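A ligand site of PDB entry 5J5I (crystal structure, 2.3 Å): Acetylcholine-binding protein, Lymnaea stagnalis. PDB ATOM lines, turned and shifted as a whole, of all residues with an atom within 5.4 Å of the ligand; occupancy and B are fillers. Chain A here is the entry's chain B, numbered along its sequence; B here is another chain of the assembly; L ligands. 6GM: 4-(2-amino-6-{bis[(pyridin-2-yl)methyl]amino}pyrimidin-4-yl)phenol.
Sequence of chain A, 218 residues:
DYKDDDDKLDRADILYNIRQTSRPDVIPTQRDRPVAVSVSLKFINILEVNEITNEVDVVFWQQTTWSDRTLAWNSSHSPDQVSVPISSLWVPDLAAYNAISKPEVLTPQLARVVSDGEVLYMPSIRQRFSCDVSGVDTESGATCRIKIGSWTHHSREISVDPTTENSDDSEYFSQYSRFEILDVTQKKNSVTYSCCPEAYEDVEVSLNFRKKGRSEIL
The side-chain hydroxyl of Thr 65 lies within hydrogen-bond range of an oxygen (O01) of the ligand (3.2 Å).
A nitrogen (N01) of the ligand is in hydrogen-bond range of the side-chain hydroxyl (OH) of Tyr 172 (3.0 Å).
The side-chain sulfur (SG) of Cys 195 of chain B lies close to a nitrogen (N01) of the ligand (3.7 Å).
The side-chain amide nitrogen (NE2) of Gln 63 lies close to a nitrogen (N03) of the ligand (3.1 Å).
O of Thr 65 lies within hydrogen-bond range of N of Ser 38 (2.9 Å).
The backbone carbonyl oxygen of Arg 112 is in hydrogen-bond range of the backbone NH of Leu 120, 2.8 Å away.
The backbone carbonyl oxygen of Met 122 lies within hydrogen-bond range of the indole nitrogen of Trp 151 of chain B.
The guanidinium group (NH1) of Arg 112 is in hydrogen-bond range of the backbone carbonyl oxygen (O) of Thr 152 of chain B (3.1 Å).
The backbone carbonyl oxygen (O) of Ser 150 of chain B is in hydrogen-bond range of the side-chain hydroxyl (OH) of Tyr 97 of chain B, at 2.9 Å.
N of Thr 152 of chain B lies within hydrogen-bond range of OG of Ser 150 of chain B, at 3.4 Å.
The backbone carbonyl oxygen of Thr 64 is in hydrogen-bond range of the backbone NH of Tyr 121, at 2.8 Å.
The side-chain sulfur (SG) of Cys 196 of chain B is disulfide-bonded to the side-chain sulfur (SG) of Cys 195 of chain B (2.1 Å).
A nitrogen (N03) of the ligand sits close to the side-chain sulfur (SD) of Met 122.
O of Trp 151 of chain B sits close to N05 of the ligand (3.1 Å).
SG of Cys 196 of chain B sits close to N03 of the ligand, 3.4 Å away.
Thr 64 touches the ligand (C to O01, 3.8 Å).
CG of Arg 112 touches C13 of the ligand, 3.6 Å away.
O of Leu 120 touches C14 of the ligand, 3.5 Å away.
Tyr 97 of chain B touches the ligand (OH to C21, 3.95 Å).
CG2 of Thr 152 of chain B touches C15 of the ligand, at 3.9 Å.
Tyr 193 of chain B touches the ligand (CD2 to N01, 3.5 Å).
Tyr 200 of chain B touches the ligand.
Hydrophobic or aromatic side chains that line the ligand: Leu 120, Met 122, Tyr 172, Tyr 97 of chain B, Trp 151 of chain B, Tyr 193 of chain B and Tyr 200 of chain B.
Within 4 Å of the ligand: Gln 63, Thr 64, Thr 65, Arg 112, Leu 120, Met 122, Tyr 172, Tyr 97 of chain B, Trp 151 of chain B, Thr 152 of chain B, Tyr 193 of chain B, Cys 195 of chain B, Cys 196 of chain B and Tyr 200 of chain B.
The nearest printed residue that does not touch the ligand is Leu 110 (4.1 Å).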
ATOM      1  N   SER A  38       8.917  -0.582   9.910  1.00  0.00           N
ATOM      2  CA  SER A  38       8.027  -1.513  10.601  1.00  0.00           C
ATOM      3  C   SER A  38       8.749  -2.115  11.797  1.00  0.00           C
ATOM      4  O   SER A  38       9.866  -2.644  11.673  1.00  0.00           O
ATOM      5  CB  SER A  38       7.559  -2.620   9.645  1.00  0.00           C
ATOM      6  OG  SER A  38       7.076  -2.079   8.431  1.00  0.00           O
ATOM      7  N   TRP A  61      12.773  -9.882  21.124  1.00  0.00           N
ATOM      8  CA  TRP A  61      13.346  -9.780  19.805  1.00  0.00           C
ATOM      9  C   TRP A  61      12.653  -8.605  19.109  1.00  0.00           C
ATOM     10  O   TRP A  61      11.435  -8.606  18.920  1.00  0.00           O
ATOM     11  CB  TRP A  61      13.164 -11.076  19.015  1.00  0.00           C
ATOM     12  CG  TRP A  61      13.826 -12.278  19.643  1.00  0.00           C
ATOM     13  CD1 TRP A  61      14.585 -12.302  20.773  1.00  0.00           C
ATOM     14  CD2 TRP A  61      13.769 -13.627  19.162  1.00  0.00           C
ATOM     15  NE1 TRP A  61      15.010 -13.579  21.021  1.00  0.00           N
ATOM     16  CE2 TRP A  61      14.529 -14.412  20.056  1.00  0.00           C
ATOM     17  CE3 TRP A  61      13.171 -14.252  18.058  1.00  0.00           C
ATOM     18  CZ2 TRP A  61      14.702 -15.797  19.883  1.00  0.00           C
ATOM     19  CZ3 TRP A  61      13.336 -15.615  17.892  1.00  0.00           C
ATOM     20  CH2 TRP A  61      14.095 -16.374  18.804  1.00  0.00           C
ATOM     21  N   GLN A  63      11.737  -7.132  16.080  1.00  0.00           N
ATOM     22  CA  GLN A  63      11.573  -7.358  14.667  1.00  0.00           C
ATOM     23  C   GLN A  63      11.503  -6.003  14.009  1.00  0.00           C
ATOM     24  O   GLN A  63      10.638  -5.196  14.355  1.00  0.00           O
ATOM     25  CB  GLN A  63      10.311  -8.164  14.377  1.00  0.00           C
ATOM     26  CG  GLN A  63      10.465  -9.643  14.564  1.00  0.00           C
ATOM     27  CD  GLN A  63       9.124 -10.338  14.678  1.00  0.00           C
ATOM     28  OE1 GLN A  63       8.235  -9.848  15.371  1.00  0.00           O
ATOM     29  NE2 GLN A  63       8.996 -11.502  14.054  1.00  0.00           N
ATOM     30  N   THR A  64      12.406  -5.760  13.069  1.00  0.00           N
ATOM     31  CA  THR A  64      12.535  -4.454  12.441  1.00  0.00           C
ATOM     32  C   THR A  64      12.774  -4.591  10.939  1.00  0.00           C
ATOM     33  O   THR A  64      13.651  -5.353  10.520  1.00  0.00           O
ATOM     34  CB  THR A  64      13.702  -3.661  13.086  1.00  0.00           C
ATOM     35  OG1 THR A  64      13.648  -3.795  14.515  1.00  0.00           O
ATOM     36  CG2 THR A  64      13.635  -2.195  12.737  1.00  0.00           C
ATOM     37  N   THR A  65      11.987  -3.887  10.131  1.00  0.00           N
ATOM     38  CA  THR A  65      12.194  -3.821   8.680  1.00  0.00           C
ATOM     39  C   THR A  65      12.036  -2.451   8.089  1.00  0.00           C
ATOM     40  O   THR A  65      11.259  -1.636   8.576  1.00  0.00           O
ATOM     41  CB  THR A  65      11.223  -4.694   7.894  1.00  0.00           C
ATOM     42  OG1 THR A  65       9.968  -4.754   8.582  1.00  0.00           O
ATOM     43  CG2 THR A  65      11.762  -6.029   7.684  1.00  0.00           C
ATOM     44  N   LEU A 110      23.863  -8.418  13.097  1.00  0.00           N
ATOM     45  CA  LEU A 110      23.781  -8.658  11.663  1.00  0.00           C
ATOM     46  C   LEU A 110      22.359  -8.407  11.160  1.00  0.00           C
ATOM     47  O   LEU A 110      21.382  -8.723  11.850  1.00  0.00           O
ATOM     48  CB  LEU A 110      24.193 -10.089  11.304  1.00  0.00           C
ATOM     49  CG  LEU A 110      25.614 -10.551  11.608  1.00  0.00           C
ATOM     50  CD1 LEU A 110      25.719 -12.016  11.286  1.00  0.00           C
ATOM     51  CD2 LEU A 110      26.625  -9.765  10.766  1.00  0.00           C
ATOM     52  N   ALA A 111      22.264  -7.837   9.963  1.00  0.00           N
ATOM     53  CA  ALA A 111      20.973  -7.738   9.270  1.00  0.00           C
ATOM     54  C   ALA A 111      20.995  -8.615   8.032  1.00  0.00           C
ATOM     55  O   ALA A 111      22.044  -8.970   7.507  1.00  0.00           O
ATOM     56  CB  ALA A 111      20.662  -6.311   8.887  1.00  0.00           C
ATOM     57  N   ARG A 112      19.798  -8.954   7.582  1.00  0.00           N
ATOM     58  CA  ARG A 112      19.614  -9.582   6.290  1.00  0.00           C
ATOM     59  C   ARG A 112      19.206  -8.500   5.291  1.00  0.00           C
ATOM     60  O   ARG A 112      18.319  -7.697   5.566  1.00  0.00           O
ATOM     61  CB  ARG A 112      18.551 -10.673   6.363  1.00  0.00           C
ATOM     62  CG  ARG A 112      18.952 -11.834   7.271  1.00  0.00           C
ATOM     63  CD  ARG A 112      20.054 -12.643   6.606  1.00  0.00           C
ATOM     64  NE  ARG A 112      19.533 -13.514   5.557  1.00  0.00           N
ATOM     65  CZ  ARG A 112      20.246 -14.465   4.963  1.00  0.00           C
ATOM     66  NH1 ARG A 112      21.508 -14.658   5.307  1.00  0.00           N
ATOM     67  NH2 ARG A 112      19.694 -15.230   4.021  1.00  0.00           N
ATOM     68  N   LEU A 120      16.114  -6.552   6.915  1.00  0.00           N
ATOM     69  CA  LEU A 120      15.540  -7.140   8.120  1.00  0.00           C
ATOM     70  C   LEU A 120      16.562  -7.195   9.251  1.00  0.00           C
ATOM     71  O   LEU A 120      17.609  -7.798   9.107  1.00  0.00           O
ATOM     72  CB  LEU A 120      15.021  -8.548   7.842  1.00  0.00           C
ATOM     73  CG  LEU A 120      13.958  -8.751   6.766  1.00  0.00           C
ATOM     74  CD1 LEU A 120      14.466  -9.740   5.769  1.00  0.00           C
ATOM     75  CD2 LEU A 120      12.692  -9.278   7.401  1.00  0.00           C
ATOM     76  N   TYR A 121      16.217  -6.584  10.378  1.00  0.00           N
ATOM     77  CA  TYR A 121      17.097  -6.518  11.533  1.00  0.00           C
ATOM     78  C   TYR A 121      16.340  -7.011  12.771  1.00  0.00           C
ATOM     79  O   TYR A 121      15.274  -6.502  13.068  1.00  0.00           O
ATOM     80  CB  TYR A 121      17.572  -5.077  11.725  1.00  0.00           C
ATOM     81  CG  TYR A 121      18.427  -4.826  12.941  1.00  0.00           C
ATOM     82  CD1 TYR A 121      19.549  -5.599  13.209  1.00  0.00           C
ATOM     83  CD2 TYR A 121      18.141  -3.764  13.803  1.00  0.00           C
ATOM     84  CE1 TYR A 121      20.346  -5.367  14.313  1.00  0.00           C
ATOM     85  CE2 TYR A 121      18.937  -3.510  14.909  1.00  0.00           C
ATOM     86  CZ  TYR A 121      20.034  -4.322  15.153  1.00  0.00           C
ATOM     87  OH  TYR A 121      20.838  -4.090  16.252  1.00  0.00           O
ATOM     88  N   MET A 122      16.883  -7.997  13.501  1.00  0.00           N
ATOM     89  CA  MET A 122      16.179  -8.469  14.691  1.00  0.00           C
ATOM     90  C   MET A 122      17.098  -8.787  15.873  1.00  0.00           C
ATOM     91  O   MET A 122      17.397  -9.948  16.172  1.00  0.00           O
ATOM     92  CB  MET A 122      15.323  -9.714  14.372  1.00  0.00           C
ATOM     93  CG  MET A 122      14.380 -10.141  15.542  1.00  0.00           C
ATOM     94  SD  MET A 122      13.461 -11.670  15.206  1.00  0.00           S
ATOM     95  CE  MET A 122      14.789 -12.827  14.828  1.00  0.00           C
ATOM     96  N   TYR A 172       7.231 -17.462  20.927  1.00  0.00           N
ATOM     97  CA  TYR A 172       8.426 -16.766  21.405  1.00  0.00           C
ATOM     98  C   TYR A 172       8.657 -16.838  22.913  1.00  0.00           C
ATOM     99  O   TYR A 172       9.758 -17.161  23.354  1.00  0.00           O
ATOM    100  CB  TYR A 172       8.358 -15.299  20.961  1.00  0.00           C
ATOM    101  CG  TYR A 172       8.361 -15.190  19.451  1.00  0.00           C
ATOM    102  CD1 TYR A 172       9.556 -15.159  18.740  1.00  0.00           C
ATOM    103  CD2 TYR A 172       7.169 -15.181  18.742  1.00  0.00           C
ATOM    104  CE1 TYR A 172       9.548 -15.090  17.361  1.00  0.00           C
ATOM    105  CE2 TYR A 172       7.162 -15.112  17.363  1.00  0.00           C
ATOM    106  CZ  TYR A 172       8.347 -15.055  16.676  1.00  0.00           C
ATOM    107  OH  TYR A 172       8.331 -14.986  15.302  1.00  0.00           O
ATOM    108  N   TYR B  97      19.386 -19.288  21.794  1.00  0.00           N
ATOM    109  CA  TYR B  97      18.039 -18.770  21.591  1.00  0.00           C
ATOM    110  C   TYR B  97      17.333 -18.503  22.921  1.00  0.00           C
ATOM    111  O   TYR B  97      16.375 -17.738  22.968  1.00  0.00           O
ATOM    112  CB  TYR B  97      17.201 -19.747  20.730  1.00  0.00           C
ATOM    113  CG  TYR B  97      17.696 -19.947  19.295  1.00  0.00           C
ATOM    114  CD1 TYR B  97      18.726 -19.171  18.764  1.00  0.00           C
ATOM    115  CD2 TYR B  97      17.116 -20.912  18.468  1.00  0.00           C
ATOM    116  CE1 TYR B  97      19.173 -19.354  17.440  1.00  0.00           C
ATOM    117  CE2 TYR B  97      17.546 -21.095  17.154  1.00  0.00           C
ATOM    118  CZ  TYR B  97      18.570 -20.312  16.633  1.00  0.00           C
ATOM    119  OH  TYR B  97      19.016 -20.491  15.326  1.00  0.00           O
ATOM    120  N   SER B 150      22.663 -20.487  14.304  1.00  0.00           N
ATOM    121  CA  SER B 150      22.902 -19.252  13.569  1.00  0.00           C
ATOM    122  C   SER B 150      21.773 -18.277  13.803  1.00  0.00           C
ATOM    123  O   SER B 150      20.601 -18.654  13.805  1.00  0.00           O
ATOM    124  CB  SER B 150      23.055 -19.518  12.075  1.00  0.00           C
ATOM    125  OG  SER B 150      23.191 -18.310  11.362  1.00  0.00           O
ATOM    126  N   TRP B 151      22.111 -17.014  14.014  1.00  0.00           N
ATOM    127  CA  TRP B 151      21.090 -15.978  14.179  1.00  0.00           C
ATOM    128  C   TRP B 151      20.469 -15.504  12.856  1.00  0.00           C
ATOM    129  O   TRP B 151      19.308 -15.095  12.830  1.00  0.00           O
ATOM    130  CB  TRP B 151      21.662 -14.774  14.927  1.00  0.00           C
ATOM    131  CG  TRP B 151      20.604 -13.838  15.405  1.00  0.00           C
ATOM    132  CD1 TRP B 151      20.420 -12.535  15.033  1.00  0.00           C
ATOM    133  CD2 TRP B 151      19.573 -14.138  16.347  1.00  0.00           C
ATOM    134  NE1 TRP B 151      19.339 -12.001  15.702  1.00  0.00           N
ATOM    135  CE2 TRP B 151      18.799 -12.967  16.514  1.00  0.00           C
ATOM    136  CE3 TRP B 151      19.228 -15.286  17.086  1.00  0.00           C
ATOM    137  CZ2 TRP B 151      17.703 -12.911  17.385  1.00  0.00           C
ATOM    138  CZ3 TRP B 151      18.136 -15.225  17.945  1.00  0.00           C
ATOM    139  CH2 TRP B 151      17.390 -14.048  18.083  1.00  0.00           C
ATOM    140  N   THR B 152      21.225 -15.559  11.765  1.00  0.00           N
ATOM    141  CA  THR B 152      20.774 -14.948  10.510  1.00  0.00           C
ATOM    142  C   THR B 152      20.898 -15.850   9.284  1.00  0.00           C
ATOM    143  O   THR B 152      20.529 -15.438   8.170  1.00  0.00           O
ATOM    144  CB  THR B 152      21.556 -13.663  10.188  1.00  0.00           C
ATOM    145  OG1 THR B 152      22.922 -13.993   9.847  1.00  0.00           O
ATOM    146  CG2 THR B 152      21.526 -12.692  11.359  1.00  0.00           C
ATOM    147  N   VAL B 191      14.203 -25.021  13.554  1.00  0.00           N
ATOM    148  CA  VAL B 191      13.320 -24.012  14.106  1.00  0.00           C
ATOM    149  C   VAL B 191      12.769 -23.114  13.004  1.00  0.00           C
ATOM    150  O   VAL B 191      13.519 -22.602  12.169  1.00  0.00           O
ATOM    151  CB  VAL B 191      14.067 -23.148  15.155  1.00  0.00           C
ATOM    152  CG1 VAL B 191      13.327 -21.873  15.439  1.00  0.00           C
ATOM    153  CG2 VAL B 191      14.287 -23.945  16.431  1.00  0.00           C
ATOM    154  N   TYR B 193       9.189 -20.190  12.203  1.00  0.00           N
ATOM    155  CA  TYR B 193       8.143 -19.379  12.807  1.00  0.00           C
ATOM    156  C   TYR B 193       7.081 -19.050  11.753  1.00  0.00           C
ATOM    157  O   TYR B 193       7.373 -19.060  10.566  1.00  0.00           O
ATOM    158  CB  TYR B 193       8.709 -18.082  13.418  1.00  0.00           C
ATOM    159  CG  TYR B 193       9.733 -18.336  14.507  1.00  0.00           C
ATOM    160  CD1 TYR B 193       9.368 -18.376  15.858  1.00  0.00           C
ATOM    161  CD2 TYR B 193      11.081 -18.564  14.179  1.00  0.00           C
ATOM    162  CE1 TYR B 193      10.314 -18.613  16.844  1.00  0.00           C
ATOM    163  CE2 TYR B 193      12.015 -18.801  15.146  1.00  0.00           C
ATOM    164  CZ  TYR B 193      11.640 -18.830  16.483  1.00  0.00           C
ATOM    165  OH  TYR B 193      12.606 -19.075  17.423  1.00  0.00           O
ATOM    166  N   CYS B 195       5.724 -16.355  10.925  1.00  0.00           N
ATOM    167  CA  CYS B 195       6.117 -15.166  10.169  1.00  0.00           C
ATOM    168  C   CYS B 195       7.101 -15.486   9.036  1.00  0.00           C
ATOM    169  O   CYS B 195       7.112 -14.837   7.990  1.00  0.00           O
ATOM    170  CB  CYS B 195       6.769 -14.132  11.094  1.00  0.00           C
ATOM    171  SG  CYS B 195       8.520 -14.510  11.475  1.00  0.00           S
ATOM    172  N   CYS B 196       7.948 -16.486   9.271  1.00  0.00           N
ATOM    173  CA  CYS B 196       9.113 -16.693   8.429  1.00  0.00           C
ATOM    174  C   CYS B 196       9.316 -18.174   8.130  1.00  0.00           C
ATOM    175  O   CYS B 196       9.565 -18.956   9.039  1.00  0.00           O
ATOM    176  CB  CYS B 196      10.364 -16.110   9.123  1.00  0.00           C
ATOM    177  SG  CYS B 196      10.021 -14.587  10.065  1.00  0.00           S
ATOM    178  N   TYR B 200      15.761 -22.875  10.557  1.00  0.00           N
ATOM    179  CA  TYR B 200      17.017 -22.531  11.193  1.00  0.00           C
ATOM    180  C   TYR B 200      17.483 -23.702  12.038  1.00  0.00           C
ATOM    181  O   TYR B 200      16.786 -24.148  12.939  1.00  0.00           O
ATOM    182  CB  TYR B 200      16.859 -21.269  12.042  1.00  0.00           C
ATOM    183  CG  TYR B 200      16.955 -20.016  11.193  1.00  0.00           C
ATOM    184  CD1 TYR B 200      16.009 -19.755  10.209  1.00  0.00           C
ATOM    185  CD2 TYR B 200      17.993 -19.105  11.356  1.00  0.00           C
ATOM    186  CE1 TYR B 200      16.091 -18.626   9.407  1.00  0.00           C
ATOM    187  CE2 TYR B 200      18.084 -17.963  10.570  1.00  0.00           C
ATOM    188  CZ  TYR B 200      17.127 -17.734   9.586  1.00  0.00           C
ATOM    189  OH  TYR B 200      17.200 -16.605   8.789  1.00  0.00           O
HETATM  190  C10 6GM L   1      10.237 -10.932  11.319  1.00  0.00           C
HETATM  191  C13 6GM L   1      16.589 -12.010   9.987  1.00  0.00           C
HETATM  192  C15 6GM L   1      18.013 -11.090  11.682  1.00  0.00           C
HETATM  193  C17 6GM L   1      14.945 -16.253  11.565  1.00  0.00           C
HETATM  194  C20 6GM L   1      16.685 -17.129  15.230  1.00  0.00           C
HETATM  195  C21 6GM L   1      15.956 -18.107  14.560  1.00  0.00           C
HETATM  196  C22 6GM L   1      15.381 -17.779  13.342  1.00  0.00           C
HETATM  197  C06 6GM L   1      12.535 -10.174  11.262  1.00  0.00           C
HETATM  198  C07 6GM L   1      12.081  -8.910  10.872  1.00  0.00           C
HETATM  199  C08 6GM L   1      10.713  -8.668  10.700  1.00  0.00           C
HETATM  200  O01 6GM L   1      10.285  -7.436  10.312  1.00  0.00           O
HETATM  201  C09 6GM L   1       9.802  -9.681  10.921  1.00  0.00           C
HETATM  202  C05 6GM L   1      11.607 -11.188  11.494  1.00  0.00           C
HETATM  203  C04 6GM L   1      12.027 -12.452  11.905  1.00  0.00           C
HETATM  204  C03 6GM L   1      13.171 -12.995  11.354  1.00  0.00           C
HETATM  205  N03 6GM L   1      11.328 -13.141  12.832  1.00  0.00           N
HETATM  206  C01 6GM L   1      11.732 -14.355  13.220  1.00  0.00           C
HETATM  207  N01 6GM L   1      11.045 -15.038  14.129  1.00  0.00           N
HETATM  208  N02 6GM L   1      12.836 -14.912  12.699  1.00  0.00           N
HETATM  209  C02 6GM L   1      13.569 -14.252  11.786  1.00  0.00           C
HETATM  210  N04 6GM L   1      14.663 -14.828  11.286  1.00  0.00           N
HETATM  211  C18 6GM L   1      15.528 -16.510  12.800  1.00  0.00           C
HETATM  212  N06 6GM L   1      16.240 -15.571  13.441  1.00  0.00           N
HETATM  213  C19 6GM L   1      16.834 -15.864  14.672  1.00  0.00           C
HETATM  214  C11 6GM L   1      15.530 -14.164  10.287  1.00  0.00           C
HETATM  215  C12 6GM L   1      16.362 -13.142  10.784  1.00  0.00           C
HETATM  216  N05 6GM L   1      16.953 -13.241  11.999  1.00  0.00           N
HETATM  217  C16 6GM L   1      17.782 -12.217  12.472  1.00  0.00           C
HETATM  218  C14 6GM L   1      17.414 -10.985  10.436  1.00  0.00           C
